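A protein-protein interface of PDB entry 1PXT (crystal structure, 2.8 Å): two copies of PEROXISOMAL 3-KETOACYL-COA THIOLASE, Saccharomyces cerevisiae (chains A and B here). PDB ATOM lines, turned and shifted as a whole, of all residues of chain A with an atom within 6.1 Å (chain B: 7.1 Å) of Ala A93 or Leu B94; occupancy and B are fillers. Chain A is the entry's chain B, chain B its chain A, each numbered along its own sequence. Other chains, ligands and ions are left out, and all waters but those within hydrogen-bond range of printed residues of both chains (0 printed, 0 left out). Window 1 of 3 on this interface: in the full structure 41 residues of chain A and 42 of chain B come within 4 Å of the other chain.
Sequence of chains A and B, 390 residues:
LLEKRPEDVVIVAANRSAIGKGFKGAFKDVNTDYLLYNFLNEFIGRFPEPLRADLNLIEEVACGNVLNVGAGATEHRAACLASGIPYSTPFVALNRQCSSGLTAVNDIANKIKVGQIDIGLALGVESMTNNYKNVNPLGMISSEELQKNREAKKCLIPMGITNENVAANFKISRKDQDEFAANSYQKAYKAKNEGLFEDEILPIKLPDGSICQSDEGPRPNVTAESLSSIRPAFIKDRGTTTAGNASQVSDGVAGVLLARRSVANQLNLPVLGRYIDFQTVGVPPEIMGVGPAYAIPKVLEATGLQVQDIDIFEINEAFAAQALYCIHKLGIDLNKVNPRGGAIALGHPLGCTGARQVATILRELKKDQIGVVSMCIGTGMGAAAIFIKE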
ATOM      1  N   VAL A  61      22.136   4.447  18.720  1.00  0.00           N
ATOM      2  CA  VAL A  61      23.318   3.967  18.032  1.00  0.00           C
ATOM      3  C   VAL A  61      24.204   5.121  17.588  1.00  0.00           C
ATOM      4  O   VAL A  61      23.900   5.797  16.617  1.00  0.00           O
ATOM      5  CB  VAL A  61      22.965   3.127  16.797  1.00  0.00           C
ATOM      6  CG1 VAL A  61      24.239   2.617  16.123  1.00  0.00           C
ATOM      7  CG2 VAL A  61      22.029   1.976  17.188  1.00  0.00           C
ATOM      8  N   ALA A  62      25.246   5.390  18.362  1.00  0.00           N
ATOM      9  CA  ALA A  62      26.208   6.412  18.029  1.00  0.00           C
ATOM     10  C   ALA A  62      27.271   5.677  17.205  1.00  0.00           C
ATOM     11  O   ALA A  62      27.787   4.659  17.650  1.00  0.00           O
ATOM     12  CB  ALA A  62      26.810   6.979  19.283  1.00  0.00           C
ATOM     13  N   CYS A  63      27.552   6.165  15.995  1.00  0.00           N
ATOM     14  CA  CYS A  63      28.546   5.580  15.092  1.00  0.00           C
ATOM     15  C   CYS A  63      29.590   6.645  14.683  1.00  0.00           C
ATOM     16  O   CYS A  63      29.235   7.682  14.095  1.00  0.00           O
ATOM     17  CB  CYS A  63      27.842   5.063  13.876  1.00  0.00           C
ATOM     18  SG  CYS A  63      28.842   3.920  12.957  1.00  0.00           S
ATOM     19  N   GLY A  64      30.847   6.433  15.088  1.00  0.00           N
ATOM     20  CA  GLY A  64      31.942   7.360  14.802  1.00  0.00           C
ATOM     21  C   GLY A  64      32.494   7.126  13.412  1.00  0.00           C
ATOM     22  O   GLY A  64      32.504   5.988  12.931  1.00  0.00           O
ATOM     23  N   ASN A  65      32.878   8.187  12.712  1.00  0.00           N
ATOM     24  CA  ASN A  65      33.386   8.029  11.354  1.00  0.00           C
ATOM     25  C   ASN A  65      34.004   9.326  10.949  1.00  0.00           C
ATOM     26  O   ASN A  65      33.447  10.392  11.170  1.00  0.00           O
ATOM     27  CB  ASN A  65      32.288   7.633  10.385  1.00  0.00           C
ATOM     28  CG  ASN A  65      32.811   7.372   9.002  1.00  0.00           C
ATOM     29  OD1 ASN A  65      33.206   8.277   8.292  1.00  0.00           O
ATOM     30  ND2 ASN A  65      32.835   6.125   8.616  1.00  0.00           N
ATOM     31  N   GLY A  70      29.491  13.337   5.396  1.00  0.00           N
ATOM     32  CA  GLY A  70      28.647  13.483   6.558  1.00  0.00           C
ATOM     33  C   GLY A  70      28.863  12.436   7.633  1.00  0.00           C
ATOM     34  O   GLY A  70      27.973  12.234   8.467  1.00  0.00           O
ATOM     35  N   ALA A  71      30.037  11.793   7.642  1.00  0.00           N
ATOM     36  CA  ALA A  71      30.345  10.758   8.636  1.00  0.00           C
ATOM     37  C   ALA A  71      29.460   9.506   8.486  1.00  0.00           C
ATOM     38  O   ALA A  71      29.069   8.863   9.463  1.00  0.00           O
ATOM     39  CB  ALA A  71      30.244  11.330  10.057  1.00  0.00           C
ATOM     40  N   GLY A  72      29.079   9.217   7.256  1.00  0.00           N
ATOM     41  CA  GLY A  72      28.313   8.033   6.961  1.00  0.00           C
ATOM     42  C   GLY A  72      26.952   7.803   7.541  1.00  0.00           C
ATOM     43  O   GLY A  72      26.371   6.731   7.315  1.00  0.00           O
ATOM     44  N   ALA A  73      26.344   8.826   8.113  1.00  0.00           N
ATOM     45  CA  ALA A  73      25.037   8.643   8.734  1.00  0.00           C
ATOM     46  C   ALA A  73      23.916   7.978   7.942  1.00  0.00           C
ATOM     47  O   ALA A  73      23.141   7.211   8.503  1.00  0.00           O
ATOM     48  CB  ALA A  73      24.575   9.919   9.336  1.00  0.00           C
ATOM     49  N   PHE A  91      19.673   6.829  15.708  1.00  0.00           N
ATOM     50  CA  PHE A  91      21.065   6.667  15.270  1.00  0.00           C
ATOM     51  C   PHE A  91      21.717   8.074  15.228  1.00  0.00           C
ATOM     52  O   PHE A  91      21.040   9.048  14.891  1.00  0.00           O
ATOM     53  CB  PHE A  91      21.073   6.073  13.858  1.00  0.00           C
ATOM     54  CG  PHE A  91      22.462   5.948  13.230  1.00  0.00           C
ATOM     55  CD1 PHE A  91      23.276   7.069  13.033  1.00  0.00           C
ATOM     56  CD2 PHE A  91      22.939   4.702  12.799  1.00  0.00           C
ATOM     57  CE1 PHE A  91      24.521   6.959  12.430  1.00  0.00           C
ATOM     58  CE2 PHE A  91      24.186   4.585  12.189  1.00  0.00           C
ATOM     59  CZ  PHE A  91      24.973   5.714  12.008  1.00  0.00           C
ATOM     60  N   VAL A  92      22.999   8.185  15.604  1.00  0.00           N
ATOM     61  CA  VAL A  92      23.734   9.444  15.562  1.00  0.00           C
ATOM     62  C   VAL A  92      25.116   9.195  14.970  1.00  0.00           C
ATOM     63  O   VAL A  92      25.802   8.272  15.375  1.00  0.00           O
ATOM     64  CB  VAL A  92      24.013  10.042  16.916  1.00  0.00           C
ATOM     65  CG1 VAL A  92      24.443  11.470  16.749  1.00  0.00           C
ATOM     66  CG2 VAL A  92      22.835   9.967  17.759  1.00  0.00           C
ATOM     67  N   ALA A  93      25.536  10.063  14.050  1.00  0.00           N
ATOM     68  CA  ALA A  93      26.827   9.956  13.405  1.00  0.00           C
ATOM     69  C   ALA A  93      27.699  10.933  14.161  1.00  0.00           C
ATOM     70  O   ALA A  93      27.213  11.921  14.637  1.00  0.00           O
ATOM     71  CB  ALA A  93      26.695  10.339  11.954  1.00  0.00           C
ATOM     72  N   LEU A  94      28.963  10.605  14.373  1.00  0.00           N
ATOM     73  CA  LEU A  94      29.889  11.478  15.114  1.00  0.00           C
ATOM     74  C   LEU A  94      31.274  11.386  14.480  1.00  0.00           C
ATOM     75  O   LEU A  94      31.661  10.347  13.923  1.00  0.00           O
ATOM     76  CB  LEU A  94      30.058  11.016  16.575  1.00  0.00           C
ATOM     77  CG  LEU A  94      29.059  11.168  17.724  1.00  0.00           C
ATOM     78  CD1 LEU A  94      27.821  10.298  17.621  1.00  0.00           C
ATOM     79  CD2 LEU A  94      29.825  10.813  18.962  1.00  0.00           C
ATOM     80  N   ASN A  95      32.024  12.466  14.580  1.00  0.00           N
ATOM     81  CA  ASN A  95      33.360  12.487  14.039  1.00  0.00           C
ATOM     82  C   ASN A  95      34.164  13.426  14.871  1.00  0.00           C
ATOM     83  O   ASN A  95      34.046  14.655  14.716  1.00  0.00           O
ATOM     84  CB  ASN A  95      33.412  12.973  12.578  1.00  0.00           C
ATOM     85  CG  ASN A  95      34.836  13.405  12.137  1.00  0.00           C
ATOM     86  OD1 ASN A  95      35.809  13.206  12.849  1.00  0.00           O
ATOM     87  ND2 ASN A  95      34.938  14.015  10.971  1.00  0.00           N
ATOM     88  N   VAL B  61      32.829  22.344  21.737  1.00  0.00           N
ATOM     89  CA  VAL B  61      32.074  22.927  20.658  1.00  0.00           C
ATOM     90  C   VAL B  61      31.546  21.786  19.795  1.00  0.00           C
ATOM     91  O   VAL B  61      32.283  21.183  19.024  1.00  0.00           O
ATOM     92  CB  VAL B  61      32.926  23.860  19.785  1.00  0.00           C
ATOM     93  CG1 VAL B  61      32.068  24.364  18.643  1.00  0.00           C
ATOM     94  CG2 VAL B  61      33.464  25.053  20.594  1.00  0.00           C
ATOM     95  N   ALA B  62      30.294  21.416  20.000  1.00  0.00           N
ATOM     96  CA  ALA B  62      29.680  20.359  19.204  1.00  0.00           C
ATOM     97  C   ALA B  62      29.034  21.174  18.102  1.00  0.00           C
ATOM     98  O   ALA B  62      28.478  22.229  18.388  1.00  0.00           O
ATOM     99  CB  ALA B  62      28.647  19.644  20.005  1.00  0.00           C
ATOM    100  N   CYS B  63      29.053  20.691  16.868  1.00  0.00           N
ATOM    101  CA  CYS B  63      28.528  21.469  15.774  1.00  0.00           C
ATOM    102  C   CYS B  63      27.931  20.603  14.691  1.00  0.00           C
ATOM    103  O   CYS B  63      28.646  19.996  13.895  1.00  0.00           O
ATOM    104  CB  CYS B  63      29.686  22.319  15.213  1.00  0.00           C
ATOM    105  SG  CYS B  63      29.451  23.079  13.584  1.00  0.00           S
ATOM    106  N   GLY B  64      26.612  20.566  14.623  1.00  0.00           N
ATOM    107  CA  GLY B  64      25.976  19.734  13.619  1.00  0.00           C
ATOM    108  C   GLY B  64      26.299  20.181  12.214  1.00  0.00           C
ATOM    109  O   GLY B  64      26.646  21.326  11.957  1.00  0.00           O
ATOM    110  N   ASN B  65      26.191  19.239  11.303  1.00  0.00           N
ATOM    111  CA  ASN B  65      26.437  19.450   9.900  1.00  0.00           C
ATOM    112  C   ASN B  65      25.987  18.119   9.317  1.00  0.00           C
ATOM    113  O   ASN B  65      26.124  17.074   9.936  1.00  0.00           O
ATOM    114  CB  ASN B  65      27.905  19.728   9.633  1.00  0.00           C
ATOM    115  CG  ASN B  65      28.180  20.083   8.181  1.00  0.00           C
ATOM    116  OD1 ASN B  65      27.921  19.279   7.279  1.00  0.00           O
ATOM    117  ND2 ASN B  65      28.687  21.287   7.941  1.00  0.00           N
ATOM    118  N   VAL B  66      25.459  18.160   8.111  1.00  0.00           N
ATOM    119  CA  VAL B  66      24.887  16.992   7.489  1.00  0.00           C
ATOM    120  C   VAL B  66      25.508  16.557   6.172  1.00  0.00           C
ATOM    121  O   VAL B  66      25.550  15.367   5.887  1.00  0.00           O
ATOM    122  CB  VAL B  66      23.339  17.311   7.224  1.00  0.00           C
ATOM    123  CG1 VAL B  66      22.562  16.130   6.611  1.00  0.00           C
ATOM    124  CG2 VAL B  66      22.685  17.786   8.488  1.00  0.00           C
ATOM    125  N   GLY B  70      32.742  14.127   6.266  1.00  0.00           N
ATOM    126  CA  GLY B  70      32.959  13.925   7.689  1.00  0.00           C
ATOM    127  C   GLY B  70      32.294  15.046   8.476  1.00  0.00           C
ATOM    128  O   GLY B  70      32.856  15.512   9.484  1.00  0.00           O
ATOM    129  N   ALA B  71      31.107  15.483   8.010  1.00  0.00           N
ATOM    130  CA  ALA B  71      30.334  16.574   8.635  1.00  0.00           C
ATOM    131  C   ALA B  71      31.192  17.766   8.971  1.00  0.00           C
ATOM    132  O   ALA B  71      31.112  18.308  10.071  1.00  0.00           O
ATOM    133  CB  ALA B  71      29.637  16.108   9.877  1.00  0.00           C
ATOM    134  N   PHE B  91      36.400  19.945  20.188  1.00  0.00           N
ATOM    135  CA  PHE B  91      35.375  20.191  19.168  1.00  0.00           C
ATOM    136  C   PHE B  91      34.805  18.831  18.748  1.00  0.00           C
ATOM    137  O   PHE B  91      35.527  17.849  18.762  1.00  0.00           O
ATOM    138  CB  PHE B  91      36.074  20.896  17.977  1.00  0.00           C
ATOM    139  CG  PHE B  91      35.211  21.083  16.764  1.00  0.00           C
ATOM    140  CD1 PHE B  91      34.998  20.040  15.881  1.00  0.00           C
ATOM    141  CD2 PHE B  91      34.594  22.295  16.517  1.00  0.00           C
ATOM    142  CE1 PHE B  91      34.167  20.204  14.775  1.00  0.00           C
ATOM    143  CE2 PHE B  91      33.766  22.462  15.419  1.00  0.00           C
ATOM    144  CZ  PHE B  91      33.554  21.424  14.554  1.00  0.00           C
ATOM    145  N   VAL B  92      33.527  18.769  18.378  1.00  0.00           N
ATOM    146  CA  VAL B  92      32.884  17.509  17.946  1.00  0.00           C
ATOM    147  C   VAL B  92      31.946  17.819  16.782  1.00  0.00           C
ATOM    148  O   VAL B  92      31.112  18.706  16.905  1.00  0.00           O
ATOM    149  CB  VAL B  92      31.888  16.924  19.003  1.00  0.00           C
ATOM    150  CG1 VAL B  92      31.944  15.406  19.001  1.00  0.00           C
ATOM    151  CG2 VAL B  92      32.045  17.550  20.367  1.00  0.00           C
ATOM    152  N   ALA B  93      31.977  17.030  15.725  1.00  0.00           N
ATOM    153  CA  ALA B  93      31.088  17.263  14.613  1.00  0.00           C
ATOM    154  C   ALA B  93      30.051  16.159  14.682  1.00  0.00           C
ATOM    155  O   ALA B  93      30.414  14.983  14.801  1.00  0.00           O
ATOM    156  CB  ALA B  93      31.851  17.182  13.325  1.00  0.00           C
ATOM    157  N   LEU B  94      28.770  16.520  14.636  1.00  0.00           N
ATOM    158  CA  LEU B  94      27.683  15.534  14.730  1.00  0.00           C
ATOM    159  C   LEU B  94      26.778  15.636  13.517  1.00  0.00           C
ATOM    160  O   LEU B  94      26.722  16.664  12.861  1.00  0.00           O
ATOM    161  CB  LEU B  94      26.829  15.745  15.999  1.00  0.00           C
ATOM    162  CG  LEU B  94      27.460  15.606  17.400  1.00  0.00           C
ATOM    163  CD1 LEU B  94      28.467  16.696  17.615  1.00  0.00           C
ATOM    164  CD2 LEU B  94      26.401  15.735  18.467  1.00  0.00           C
ATOM    165  N   ASN B  95      26.134  14.538  13.167  1.00  0.00           N
ATOM    166  CA  ASN B  95      25.197  14.522  12.066  1.00  0.00           C
ATOM    167  C   ASN B  95      24.016  13.616  12.405  1.00  0.00           C
ATOM    168  O   ASN B  95      24.131  12.370  12.362  1.00  0.00           O
ATOM    169  CB  ASN B  95      25.807  14.060  10.741  1.00  0.00           C
ATOM    170  CG  ASN B  95      24.753  13.903   9.645  1.00  0.00           C
ATOM    171  OD1 ASN B  95      23.640  14.361   9.801  1.00  0.00           O
ATOM    172  ND2 ASN B  95      25.098  13.271   8.547  1.00  0.00           N
ATOM    173  N   ARG B  96      22.910  14.256  12.802  1.00  0.00           N
ATOM    174  CA  ARG B  96      21.661  13.559  13.068  1.00  0.00           C
ATOM    175  C   ARG B  96      20.685  13.978  11.963  1.00  0.00           C
ATOM    176  O   ARG B  96      19.471  13.817  12.071  1.00  0.00           O
ATOM    177  CB  ARG B  96      21.102  13.902  14.431  1.00  0.00           C
ATOM    178  CG  ARG B  96      20.056  12.910  14.875  1.00  0.00           C
ATOM    179  CD  ARG B  96      20.096  12.850  16.365  1.00  0.00           C
ATOM    180  NE  ARG B  96      19.642  11.569  16.840  1.00  0.00           N
ATOM    181  CZ  ARG B  96      19.962  11.057  18.020  1.00  0.00           C
ATOM    182  NH1 ARG B  96      20.748  11.711  18.878  1.00  0.00           N
ATOM    183  NH2 ARG B  96      19.521   9.848  18.311  1.00  0.00           N
ATOM    184  N   GLN B  97      21.241  14.502  10.880  1.00  0.00           N
ATOM    185  CA  GLN B  97      20.455  14.931   9.740  1.00  0.00           C
ATOM    186  C   GLN B  97      19.716  16.219  10.110  1.00  0.00           C
ATOM    187  O   GLN B  97      20.303  17.140  10.694  1.00  0.00           O
ATOM    188  CB  GLN B  97      19.456  13.846   9.301  1.00  0.00           C
ATOM    189  CG  GLN B  97      20.005  12.460   9.114  1.00  0.00           C
ATOM    190  CD  GLN B  97      20.923  12.307   7.901  1.00  0.00           C
ATOM    191  OE1 GLN B  97      20.545  11.698   6.888  1.00  0.00           O
ATOM    192  NE2 GLN B  97      22.165  12.793   8.027  1.00  0.00           N
ATOM    193  N   SER B 100      20.373  17.891  13.470  1.00  0.00           N
ATOM    194  CA  SER B 100      21.773  18.086  13.869  1.00  0.00           C
ATOM    195  C   SER B 100      22.065  19.249  14.796  1.00  0.00           C
ATOM    196  O   SER B 100      22.715  19.069  15.827  1.00  0.00           O
ATOM    197  CB  SER B 100      22.691  18.038  12.649  1.00  0.00           C
ATOM    198  OG  SER B 100      22.391  16.848  11.881  1.00  0.00           O
ATOM    199  N   GLY B 101      21.505  20.414  14.506  1.00  0.00           N
ATOM    200  CA  GLY B 101      21.744  21.550  15.374  1.00  0.00           C
ATOM    201  C   GLY B 101      21.133  21.376  16.760  1.00  0.00           C
ATOM    202  O   GLY B 101      21.639  21.947  17.731  1.00  0.00           O
ATOM    203  N   THR B 103      20.486  18.252  18.270  1.00  0.00           N
ATOM    204  CA  THR B 103      21.214  17.195  18.950  1.00  0.00           C
ATOM    205  C   THR B 103      22.572  17.742  19.397  1.00  0.00           C
ATOM    206  O   THR B 103      23.129  17.302  20.409  1.00  0.00           O
ATOM    207  CB  THR B 103      21.328  15.869  18.119  1.00  0.00           C
ATOM    208  OG1 THR B 103      22.499  15.877  17.308  1.00  0.00           O
ATOM    209  CG2 THR B 103      20.144  15.710  17.226  1.00  0.00           C
ATOM    210  N   ALA B 104      23.069  18.760  18.700  1.00  0.00           N
ATOM    211  CA  ALA B 104      24.332  19.363  19.095  1.00  0.00           C
ATOM    212  C   ALA B 104      24.100  20.076  20.402  1.00  0.00           C
ATOM    213  O   ALA B 104      25.035  20.307  21.163  1.00  0.00           O
ATOM    214  CB  ALA B 104      24.803  20.326  18.058  1.00  0.00           C
ATOM    215  N   VAL B 105      22.851  20.477  20.632  1.00  0.00           N
ATOM    216  CA  VAL B 105      22.474  21.155  21.870  1.00  0.00           C
ATOM    217  C   VAL B 105      22.285  20.074  22.930  1.00  0.00           C
ATOM    218  O   VAL B 105      22.692  20.243  24.096  1.00  0.00           O
ATOM    219  CB  VAL B 105      21.174  21.989  21.702  1.00  0.00           C
ATOM    220  CG1 VAL B 105      20.709  22.515  23.039  1.00  0.00           C
ATOM    221  CG2 VAL B 105      21.431  23.150  20.746  1.00  0.00           C
ATOM    222  N   ASN B 106      21.699  18.950  22.503  1.00  0.00           N
ATOM    223  CA  ASN B 106      21.514  17.828  23.399  1.00  0.00           C
ATOM    224  C   ASN B 106      22.885  17.434  23.899  1.00  0.00           C
ATOM    225  O   ASN B 106      23.090  17.271  25.100  1.00  0.00           O
ATOM    226  CB  ASN B 106      20.911  16.642  22.682  1.00  0.00           C
ATOM    227  CG  ASN B 106      20.649  15.465  23.624  1.00  0.00           C
ATOM    228  OD1 ASN B 106      20.638  14.290  23.198  1.00  0.00           O
ATOM    229  ND2 ASN B 106      20.421  15.773  24.906  1.00  0.00           N
ATOM    230  N   ASP B 107      23.839  17.358  22.976  1.00  0.00           N
ATOM    231  CA  ASP B 107      25.196  17.005  23.311  1.00  0.00           C
ATOM    232  C   ASP B 107      25.718  17.857  24.426  1.00  0.00           C
ATOM    233  O   ASP B 107      26.122  17.338  25.447  1.00  0.00           O
ATOM    234  CB  ASP B 107      26.132  17.136  22.093  1.00  0.00           C
ATOM    235  CG  ASP B 107      27.618  16.979  22.474  1.00  0.00           C
ATOM    236  OD1 ASP B 107      28.051  15.862  22.777  1.00  0.00           O
ATOM    237  OD2 ASP B 107      28.369  17.966  22.475  1.00  0.00           O
ATOM    238  N   ILE B 108      25.682  19.173  24.239  1.00  0.00           N
ATOM    239  CA  ILE B 108      26.235  20.103  25.238  1.00  0.00           C
ATOM    240  C   ILE B 108      25.528  20.019  26.600  1.00  0.00           C
ATOM    241  O   ILE B 108      26.172  20.010  27.668  1.00  0.00           O
ATOM    242  CB  ILE B 108      26.317  21.546  24.651  1.00  0.00           C
ATOM    243  CG1 ILE B 108      27.276  21.540  23.458  1.00  0.00           C
ATOM    244  CG2 ILE B 108      26.895  22.515  25.653  1.00  0.00           C
ATOM    245  CD1 ILE B 108      28.748  21.247  23.846  1.00  0.00           C
ATOM    246  N   LYS B 111      26.698  16.758  28.615  1.00  0.00           N
ATOM    247  CA  LYS B 111      28.035  16.897  29.179  1.00  0.00           C
ATOM    248  C   LYS B 111      28.014  17.797  30.405  1.00  0.00           C
ATOM    249  O   LYS B 111      28.750  17.570  31.379  1.00  0.00           O
ATOM    250  CB  LYS B 111      29.011  17.418  28.121  1.00  0.00           C
ATOM    251  CG  LYS B 111      29.098  16.504  26.923  1.00  0.00           C
ATOM    252  CD  LYS B 111      29.723  17.134  25.706  1.00  0.00           C
ATOM    253  CE  LYS B 111      30.349  16.030  24.860  1.00  0.00           C
ATOM    254  NZ  LYS B 111      30.673  16.394  23.460  1.00  0.00           N
ATOM    255  N   GLY B 351      21.499  21.223   8.751  1.00  0.00           N
ATOM    256  CA  GLY B 351      22.072  21.108  10.074  1.00  0.00           C
ATOM    257  C   GLY B 351      22.018  22.335  10.938  1.00  0.00           C
ATOM    258  O   GLY B 351      22.453  22.314  12.094  1.00  0.00           O
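ND2 of Asn B95 sits at hydrogen-bond distance from O of Val B66 (3.4 Å). The backbone NH (N) of Gln B97 is in hydrogen-bond range of the side-chain amide oxygen (OD1) of Asn B95, at 2.6 Å. The side-chain amide oxygen of Asn B95 lies within hydrogen-bond range of the side-chain hydroxyl of Ser B100. N of Arg B96 is in hydrogen-bond range of OG of Ser B100 (2.8 Å). The side-chain hydroxyl of Ser B100 sits at hydrogen-bond distance from the backbone carbonyl oxygen of Gln B97 (2.4 Å). The backbone carbonyl oxygen of Cys A63 sits at hydrogen-bond distance from the backbone NH of Leu A94.
Gly A70 touches its own counterpart, Gly B70. Gly A70 touches Asn B95, and with the chains exchanged Asn A95 touches Gly B70. Ala A93 touches Leu B94, and with the chains exchanged Leu A94 touches Ala B93. Ala A93 touches Asn B95, and with the chains exchanged Asn A95 touches Ala B93. Of the 15 pairs that touch across the chains among the printed residues, 10 have their exchanged pair printed and touching as well.
Of chain B, only Leu B94 (3.6 Å) and Asn B95 (3.2 Å) come within 4 Å of Ala A93. Printed residues of chain A within 4 Å of Leu B94: Ala A93. Of the printed residues of chain B, Ala A73 touches Asn B95 (3.5 Å) and Gln B97 (3.97 Å). Printed residues of chain A within 4 Å of Asn B95: Gly A70, Ala A73 and Ala A93. Printed residues of chain B within 4 Å of Val A92: Arg B96.
The backbone carbonyl oxygen (O) of Gly B70 sits at hydrogen-bond distance from the side-chain amide nitrogen (ND2) of Asn A95 (3.0 Å). The backbone carbonyl oxygen (O) of Ala B93 is in hydrogen-bond range of the backbone NH (N) of Asn A95. ND2 of Asn B95 lies within hydrogen-bond range of O of Gly A70. N of Ala A93 sits at hydrogen-bond distance from O of Asn B95, 3.2 Å away. The guanidinium group (NE) of Arg B96 is in hydrogen-bond range of the backbone carbonyl oxygen (O) of Phe A91, at 3.5 Å. N of Gly B70 sits close to N of Gly A70 (3.5 Å).
Printed residues of chain A that touch a printed residue of chain B: Gly A70, Ala A71, Ala A73, Phe A91, Val A92, Ala A93, Leu A94 and Asn A95. Hydrophobic or aromatic side chains of chain B that line the printed part of chain A: Ala B93. Among the printed residues, 15 pairs touch across the chains. Among the printed residues, no Asp or Glu carboxylate lies within 4 Å of a Lys or Arg side-chain nitrogen of the other chain.
Among the printed residues, merely in contact across the chains: Gly A70 with Val B66 (3.7 Å), Gly A70 with Ala B71 (3.5 Å), Ala A71 with Gly B70 (3.6 Å), Ala A71 with Ala B71 (3.9 Å), Ala A73 with Asn B95 (3.5 Å), Ala A73 with Gln B97 (3.97 Å), Val A92 with Arg B96 (2.9 Å), Ala A93 with Leu B94 (3.6 Å) and Leu A94 with Ala B93 (3.6 Å).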
